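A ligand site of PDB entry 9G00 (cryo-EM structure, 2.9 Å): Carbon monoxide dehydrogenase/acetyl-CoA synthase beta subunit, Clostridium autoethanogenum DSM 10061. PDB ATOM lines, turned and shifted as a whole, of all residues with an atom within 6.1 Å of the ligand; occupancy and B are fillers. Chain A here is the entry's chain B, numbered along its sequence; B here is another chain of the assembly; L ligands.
A ring nitrogen (NE2) of His 258 binds an iron atom (FE2) of the ligand (2.1 Å). The side-chain sulfur (SG) of Cys 522 binds a nickel atom (NI1) of the ligand (2.1 Å). A sulfur (S1) of the ligand sits close to the backbone NH (N) of Cys 480 (3.6 Å). The side-chain sulfur (SG) of Cys 480 is bound to an iron atom (FE4) of the ligand (2.2 Å). An iron atom (FE2) of the ligand is bound by the side-chain sulfur (SG) of Cys 294 (2.3 Å). N of Cys 450 sits close to S1 of the ligand, at 3.8 Å. An iron atom (FE3) of the ligand is bound by the side-chain sulfur of Cys 450, 2.3 Å away. FE1 of the ligand is bound by SG of Cys 332. A sulfur (S3) of the ligand sits close to the side-chain hydroxyl of Ser 557 (3.1 Å). S3 of the ligand sits close to NZ of Lys 559 (3.5 Å).
NE2 of His 258 sits close to NZ of Lys 559 (2.8 Å). The backbone carbonyl oxygen (O) of Cys 480 sits at hydrogen-bond distance from the side-chain amide nitrogen (ND2) of Asn 310. The backbone carbonyl oxygen (O) of Gly 257 is in hydrogen-bond range of the backbone NH (N) of Cys 294, 3.5 Å away. SG of Cys 450 sits close to OG of Ser 557 (3.6 Å). The backbone NH of Met 556 sits close to the side-chain sulfur of Cys 450 (3.3 Å). The backbone carbonyl oxygen (O) of Gly 449 lies within hydrogen-bond range of the backbone NH (N) of Ala 481 (3.2 Å). The backbone NH (N) of Phe 311 is in hydrogen-bond range of the side-chain sulfur (SG) of Cys 293, at 3.6 Å. NZ of Lys 559 is in hydrogen-bond range of OE1 of Gln 331, 2.7 Å away.
The backbone carbonyl oxygen (O) of Gly 449 sits close to a sulfur (S1) of the ligand, at 3.4 Å. Cys 293 touches the ligand (CB to S4, 3.7 Å). Phe 311 touches the ligand (CB to S2, 3.4 Å). CE of Met 556 touches S2 of the ligand, 3.7 Å away. Of the 26 residues printed, 12 come within 4 Å of the ligand. The nearest printed residue that does not touch the ligand is Gly 479 (4.3 Å).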
ATOM      1  N   HIS A  92     -13.323   1.374 -28.509  1.00  0.00           N
ATOM      2  CA  HIS A  92     -14.241   2.481 -28.784  1.00  0.00           C
ATOM      3  C   HIS A  92     -15.141   2.199 -29.982  1.00  0.00           C
ATOM      4  O   HIS A  92     -16.343   2.490 -29.959  1.00  0.00           O
ATOM      5  CB  HIS A  92     -13.465   3.776 -28.973  1.00  0.00           C
ATOM      6  CG  HIS A  92     -13.050   4.426 -27.693  1.00  0.00           C
ATOM      7  ND1 HIS A  92     -11.856   5.087 -27.541  1.00  0.00           N
ATOM      8  CD2 HIS A  92     -13.669   4.503 -26.507  1.00  0.00           C
ATOM      9  CE1 HIS A  92     -11.756   5.533 -26.302  1.00  0.00           C
ATOM     10  NE2 HIS A  92     -12.863   5.202 -25.649  1.00  0.00           N
ATOM     11  N   GLY A 257     -19.232  -0.078 -16.155  1.00  0.00           N
ATOM     12  CA  GLY A 257     -18.983  -0.404 -17.550  1.00  0.00           C
ATOM     13  C   GLY A 257     -19.094   0.791 -18.488  1.00  0.00           C
ATOM     14  O   GLY A 257     -18.842   1.925 -18.078  1.00  0.00           O
ATOM     15  N   HIS A 258     -19.406   0.539 -19.769  1.00  0.00           N
ATOM     16  CA  HIS A 258     -19.364   1.598 -20.764  1.00  0.00           C
ATOM     17  C   HIS A 258     -20.590   1.710 -21.667  1.00  0.00           C
ATOM     18  O   HIS A 258     -20.941   2.815 -22.102  1.00  0.00           O
ATOM     19  CB  HIS A 258     -18.104   1.443 -21.620  1.00  0.00           C
ATOM     20  CG  HIS A 258     -16.844   1.798 -20.896  1.00  0.00           C
ATOM     21  ND1 HIS A 258     -16.313   1.027 -19.878  1.00  0.00           N
ATOM     22  CD2 HIS A 258     -16.030   2.871 -20.994  1.00  0.00           C
ATOM     23  CE1 HIS A 258     -15.233   1.603 -19.409  1.00  0.00           C
ATOM     24  NE2 HIS A 258     -15.033   2.732 -20.071  1.00  0.00           N
ATOM     25  N   CYS A 293     -17.683   4.789 -13.390  1.00  0.00           N
ATOM     26  CA  CYS A 293     -16.911   4.898 -14.648  1.00  0.00           C
ATOM     27  C   CYS A 293     -17.836   5.486 -15.721  1.00  0.00           C
ATOM     28  O   CYS A 293     -18.651   6.363 -15.429  1.00  0.00           O
ATOM     29  CB  CYS A 293     -16.310   3.535 -14.994  1.00  0.00           C
ATOM     30  SG  CYS A 293     -14.992   2.977 -13.878  1.00  0.00           S
ATOM     31  N   CYS A 294     -17.711   5.032 -16.967  1.00  0.00           N
ATOM     32  CA  CYS A 294     -18.335   5.724 -18.102  1.00  0.00           C
ATOM     33  C   CYS A 294     -19.841   5.494 -18.181  1.00  0.00           C
ATOM     34  O   CYS A 294     -20.571   6.391 -18.588  1.00  0.00           O
ATOM     35  CB  CYS A 294     -17.667   5.319 -19.408  1.00  0.00           C
ATOM     36  SG  CYS A 294     -16.110   6.177 -19.650  1.00  0.00           S
ATOM     37  N   ASN A 310     -14.966   6.295  -9.565  1.00  0.00           N
ATOM     38  CA  ASN A 310     -14.239   6.028 -10.806  1.00  0.00           C
ATOM     39  C   ASN A 310     -13.498   4.689 -10.721  1.00  0.00           C
ATOM     40  O   ASN A 310     -13.712   3.878  -9.813  1.00  0.00           O
ATOM     41  CB  ASN A 310     -13.326   7.207 -11.182  1.00  0.00           C
ATOM     42  CG  ASN A 310     -12.435   7.695 -10.037  1.00  0.00           C
ATOM     43  OD1 ASN A 310     -12.333   7.037  -9.011  1.00  0.00           O
ATOM     44  ND2 ASN A 310     -11.782   8.847 -10.223  1.00  0.00           N
ATOM     45  N   PHE A 311     -12.576   4.453 -11.665  1.00  0.00           N
ATOM     46  CA  PHE A 311     -11.982   3.136 -11.914  1.00  0.00           C
ATOM     47  C   PHE A 311     -11.452   2.499 -10.627  1.00  0.00           C
ATOM     48  O   PHE A 311     -11.936   1.442 -10.237  1.00  0.00           O
ATOM     49  CB  PHE A 311     -10.882   3.248 -12.973  1.00  0.00           C
ATOM     50  CG  PHE A 311     -10.158   1.955 -13.268  1.00  0.00           C
ATOM     51  CD1 PHE A 311     -10.824   0.899 -13.911  1.00  0.00           C
ATOM     52  CD2 PHE A 311      -8.819   1.798 -12.916  1.00  0.00           C
ATOM     53  CE1 PHE A 311     -10.158  -0.320 -14.196  1.00  0.00           C
ATOM     54  CE2 PHE A 311      -8.125   0.587 -13.199  1.00  0.00           C
ATOM     55  CZ  PHE A 311      -8.805  -0.473 -13.843  1.00  0.00           C
ATOM     56  N   GLN A 331     -15.452  -3.524 -20.468  1.00  0.00           N
ATOM     57  CA  GLN A 331     -14.355  -2.560 -20.409  1.00  0.00           C
ATOM     58  C   GLN A 331     -14.136  -2.020 -18.987  1.00  0.00           C
ATOM     59  O   GLN A 331     -15.084  -1.603 -18.312  1.00  0.00           O
ATOM     60  CB  GLN A 331     -14.571  -1.396 -21.390  1.00  0.00           C
ATOM     61  CG  GLN A 331     -14.618  -1.821 -22.880  1.00  0.00           C
ATOM     62  CD  GLN A 331     -14.903  -0.639 -23.810  1.00  0.00           C
ATOM     63  OE1 GLN A 331     -14.633   0.505 -23.463  1.00  0.00           O
ATOM     64  NE2 GLN A 331     -15.471  -0.905 -24.977  1.00  0.00           N
ATOM     65  N   CYS A 332     -12.878  -2.024 -18.531  1.00  0.00           N
ATOM     66  CA  CYS A 332     -12.486  -1.427 -17.240  1.00  0.00           C
ATOM     67  C   CYS A 332     -13.233  -2.055 -16.052  1.00  0.00           C
ATOM     68  O   CYS A 332     -13.436  -1.406 -15.028  1.00  0.00           O
ATOM     69  CB  CYS A 332     -12.665   0.095 -17.260  1.00  0.00           C
ATOM     70  SG  CYS A 332     -11.858   0.867 -18.673  1.00  0.00           S
ATOM     71  N   VAL A 448      -8.667  14.195 -19.099  1.00  0.00           N
ATOM     72  CA  VAL A 448      -9.300  12.912 -19.402  1.00  0.00           C
ATOM     73  C   VAL A 448      -8.425  11.809 -18.818  1.00  0.00           C
ATOM     74  O   VAL A 448      -7.291  12.049 -18.398  1.00  0.00           O
ATOM     75  CB  VAL A 448      -9.477  12.704 -20.927  1.00  0.00           C
ATOM     76  CG1 VAL A 448     -10.113  13.941 -21.556  1.00  0.00           C
ATOM     77  CG2 VAL A 448      -8.127  12.402 -21.591  1.00  0.00           C
ATOM     78  N   GLY A 449      -8.951  10.594 -18.793  1.00  0.00           N
ATOM     79  CA  GLY A 449      -8.116   9.450 -18.466  1.00  0.00           C
ATOM     80  C   GLY A 449      -8.575   8.749 -17.208  1.00  0.00           C
ATOM     81  O   GLY A 449      -9.498   9.174 -16.513  1.00  0.00           O
ATOM     82  N   CYS A 450      -7.856   7.679 -16.883  1.00  0.00           N
ATOM     83  CA  CYS A 450      -8.187   6.760 -15.816  1.00  0.00           C
ATOM     84  C   CYS A 450      -7.432   7.087 -14.535  1.00  0.00           C
ATOM     85  O   CYS A 450      -6.890   8.189 -14.381  1.00  0.00           O
ATOM     86  CB  CYS A 450      -7.763   5.355 -16.281  1.00  0.00           C
ATOM     87  SG  CYS A 450      -7.633   5.162 -18.085  1.00  0.00           S
ATOM     88  N   ASN A 451      -7.450   6.167 -13.588  1.00  0.00           N
ATOM     89  CA  ASN A 451      -6.536   6.131 -12.467  1.00  0.00           C
ATOM     90  C   ASN A 451      -5.443   5.115 -12.805  1.00  0.00           C
ATOM     91  O   ASN A 451      -5.569   4.333 -13.758  1.00  0.00           O
ATOM     92  CB  ASN A 451      -7.226   5.767 -11.159  1.00  0.00           C
ATOM     93  CG  ASN A 451      -8.366   6.707 -10.807  1.00  0.00           C
ATOM     94  OD1 ASN A 451      -9.476   6.274 -10.546  1.00  0.00           O
ATOM     95  ND2 ASN A 451      -8.085   8.023 -10.788  1.00  0.00           N
ATOM     96  N   THR A 478     -13.594  14.601 -18.790  1.00  0.00           N
ATOM     97  CA  THR A 478     -14.342  13.406 -19.152  1.00  0.00           C
ATOM     98  C   THR A 478     -13.872  12.220 -18.308  1.00  0.00           C
ATOM     99  O   THR A 478     -12.832  12.273 -17.654  1.00  0.00           O
ATOM    100  CB  THR A 478     -14.242  13.038 -20.652  1.00  0.00           C
ATOM    101  OG1 THR A 478     -12.902  12.638 -20.966  1.00  0.00           O
ATOM    102  CG2 THR A 478     -14.646  14.207 -21.530  1.00  0.00           C
ATOM    103  N   GLY A 479     -14.739  11.225 -18.206  1.00  0.00           N
ATOM    104  CA  GLY A 479     -14.349   9.942 -17.651  1.00  0.00           C
ATOM    105  C   GLY A 479     -13.992   9.971 -16.179  1.00  0.00           C
ATOM    106  O   GLY A 479     -14.597  10.672 -15.363  1.00  0.00           O
ATOM    107  N   CYS A 480     -12.986   9.163 -15.840  1.00  0.00           N
ATOM    108  CA  CYS A 480     -12.592   9.029 -14.441  1.00  0.00           C
ATOM    109  C   CYS A 480     -11.982  10.319 -13.898  1.00  0.00           C
ATOM    110  O   CYS A 480     -12.100  10.609 -12.704  1.00  0.00           O
ATOM    111  CB  CYS A 480     -11.631   7.837 -14.299  1.00  0.00           C
ATOM    112  SG  CYS A 480     -12.504   6.237 -14.470  1.00  0.00           S
ATOM    113  N   ALA A 481     -11.327  11.117 -14.751  1.00  0.00           N
ATOM    114  CA  ALA A 481     -10.886  12.451 -14.341  1.00  0.00           C
ATOM    115  C   ALA A 481     -12.063  13.335 -13.979  1.00  0.00           C
ATOM    116  O   ALA A 481     -12.055  14.016 -12.953  1.00  0.00           O
ATOM    117  CB  ALA A 481     -10.049  13.098 -15.457  1.00  0.00           C
ATOM    118  N   GLN A 483     -14.900  12.287 -12.896  1.00  0.00           N
ATOM    119  CA  GLN A 483     -15.429  11.778 -11.626  1.00  0.00           C
ATOM    120  C   GLN A 483     -14.533  12.163 -10.456  1.00  0.00           C
ATOM    121  O   GLN A 483     -15.040  12.452  -9.363  1.00  0.00           O
ATOM    122  CB  GLN A 483     -15.669  10.269 -11.746  1.00  0.00           C
ATOM    123  CG  GLN A 483     -16.802   9.947 -12.755  1.00  0.00           C
ATOM    124  CD  GLN A 483     -17.024   8.447 -13.030  1.00  0.00           C
ATOM    125  OE1 GLN A 483     -16.149   7.636 -12.790  1.00  0.00           O
ATOM    126  NE2 GLN A 483     -18.209   8.104 -13.545  1.00  0.00           N
ATOM    127  N   SER A 521     -18.602  10.891 -20.901  1.00  0.00           N
ATOM    128  CA  SER A 521     -17.774   9.689 -20.812  1.00  0.00           C
ATOM    129  C   SER A 521     -16.564   9.810 -21.733  1.00  0.00           C
ATOM    130  O   SER A 521     -16.294  10.848 -22.317  1.00  0.00           O
ATOM    131  CB  SER A 521     -18.626   8.456 -21.131  1.00  0.00           C
ATOM    132  OG  SER A 521     -19.064   8.470 -22.484  1.00  0.00           O
ATOM    133  N   CYS A 522     -15.817   8.702 -21.863  1.00  0.00           N
ATOM    134  CA  CYS A 522     -14.616   8.701 -22.700  1.00  0.00           C
ATOM    135  C   CYS A 522     -14.960   8.887 -24.171  1.00  0.00           C
ATOM    136  O   CYS A 522     -14.279   9.628 -24.888  1.00  0.00           O
ATOM    137  CB  CYS A 522     -13.825   7.422 -22.456  1.00  0.00           C
ATOM    138  SG  CYS A 522     -13.073   7.466 -20.825  1.00  0.00           S
ATOM    139  N   MET A 556      -4.375   4.622 -17.818  1.00  0.00           N
ATOM    140  CA  MET A 556      -3.928   3.235 -17.754  1.00  0.00           C
ATOM    141  C   MET A 556      -4.282   2.409 -19.000  1.00  0.00           C
ATOM    142  O   MET A 556      -3.559   1.475 -19.329  1.00  0.00           O
ATOM    143  CB  MET A 556      -4.493   2.560 -16.478  1.00  0.00           C
ATOM    144  CG  MET A 556      -6.016   2.299 -16.499  1.00  0.00           C
ATOM    145  SD  MET A 556      -6.565   0.737 -17.221  1.00  0.00           S
ATOM    146  CE  MET A 556      -8.342   0.914 -17.168  1.00  0.00           C
ATOM    147  N   SER A 557      -5.367   2.740 -19.693  1.00  0.00           N
ATOM    148  CA  SER A 557      -5.968   1.848 -20.682  1.00  0.00           C
ATOM    149  C   SER A 557      -5.391   2.066 -22.090  1.00  0.00           C
ATOM    150  O   SER A 557      -4.895   3.156 -22.468  1.00  0.00           O
ATOM    151  CB  SER A 557      -7.503   1.999 -20.710  1.00  0.00           C
ATOM    152  OG  SER A 557      -7.896   3.291 -21.167  1.00  0.00           O
ATOM    153  N   LYS A 559      -7.377   2.333 -24.496  1.00  0.00           N
ATOM    154  CA  LYS A 559      -8.255   3.392 -24.981  1.00  0.00           C
ATOM    155  C   LYS A 559      -7.637   4.781 -24.770  1.00  0.00           C
ATOM    156  O   LYS A 559      -7.675   5.621 -25.662  1.00  0.00           O
ATOM    157  CB  LYS A 559      -9.608   3.323 -24.284  1.00  0.00           C
ATOM    158  CG  LYS A 559     -10.554   2.274 -24.872  1.00  0.00           C
ATOM    159  CD  LYS A 559     -11.914   2.272 -24.131  1.00  0.00           C
ATOM    160  CE  LYS A 559     -11.765   1.756 -22.675  1.00  0.00           C
ATOM    161  NZ  LYS A 559     -13.021   1.881 -21.846  1.00  0.00           N
ATOM    162  N   ALA A 560      -6.984   4.988 -23.623  1.00  0.00           N
ATOM    163  CA  ALA A 560      -6.315   6.262 -23.363  1.00  0.00           C
ATOM    164  C   ALA A 560      -5.205   6.503 -24.367  1.00  0.00           C
ATOM    165  O   ALA A 560      -5.023   7.637 -24.840  1.00  0.00           O
ATOM    166  CB  ALA A 560      -5.781   6.303 -21.933  1.00  0.00           C
ATOM    167  N   ILE A 563      -6.812   7.567 -27.578  1.00  0.00           N
ATOM    168  CA  ILE A 563      -7.372   8.919 -27.420  1.00  0.00           C
ATOM    169  C   ILE A 563      -6.273   9.962 -27.554  1.00  0.00           C
ATOM    170  O   ILE A 563      -6.398  10.920 -28.330  1.00  0.00           O
ATOM    171  CB  ILE A 563      -8.086   9.051 -26.064  1.00  0.00           C
ATOM    172  CG1 ILE A 563      -9.416   8.301 -26.077  1.00  0.00           C
ATOM    173  CG2 ILE A 563      -8.314  10.543 -25.687  1.00  0.00           C
ATOM    174  CD1 ILE A 563      -9.948   8.057 -24.681  1.00  0.00           C
ATOM    175  N   HIS B 194      -9.052  -6.166 -24.271  1.00  0.00           N
ATOM    176  CA  HIS B 194      -8.770  -4.915 -23.554  1.00  0.00           C
ATOM    177  C   HIS B 194      -8.955  -5.095 -22.041  1.00  0.00           C
ATOM    178  O   HIS B 194      -9.771  -5.904 -21.591  1.00  0.00           O
ATOM    179  CB  HIS B 194      -9.713  -3.824 -24.080  1.00  0.00           C
ATOM    180  CG  HIS B 194      -9.448  -2.466 -23.513  1.00  0.00           C
ATOM    181  ND1 HIS B 194      -9.857  -2.078 -22.258  1.00  0.00           N
ATOM    182  CD2 HIS B 194      -8.835  -1.378 -24.054  1.00  0.00           C
ATOM    183  CE1 HIS B 194      -9.494  -0.834 -22.032  1.00  0.00           C
ATOM    184  NE2 HIS B 194      -8.871  -0.379 -23.117  1.00  0.00           N
HETATM  185 FE1  LIG L   1     -11.818   3.152 -18.153  1.00  0.00          FE
HETATM  186 FE2  LIG L   1     -14.404   4.674 -19.712  1.00  0.00          FE
HETATM  187 FE3  LIG L   1      -9.958   5.050 -18.175  1.00  0.00          FE
HETATM  188 FE4  LIG L   1     -12.087   5.449 -16.491  1.00  0.00          FE
HETATM  189  S1  LIG L   1     -11.338   6.878 -18.155  1.00  0.00           S
HETATM  190  S2  LIG L   1     -10.464   3.785 -16.354  1.00  0.00           S
HETATM  191  S3  LIG L   1     -10.706   3.886 -20.070  1.00  0.00           S
HETATM  192  S4  LIG L   1     -13.728   4.133 -17.538  1.00  0.00           S
HETATM  193 NI1  LIG L   1     -12.174   5.773 -19.996  1.00  0.00          NI
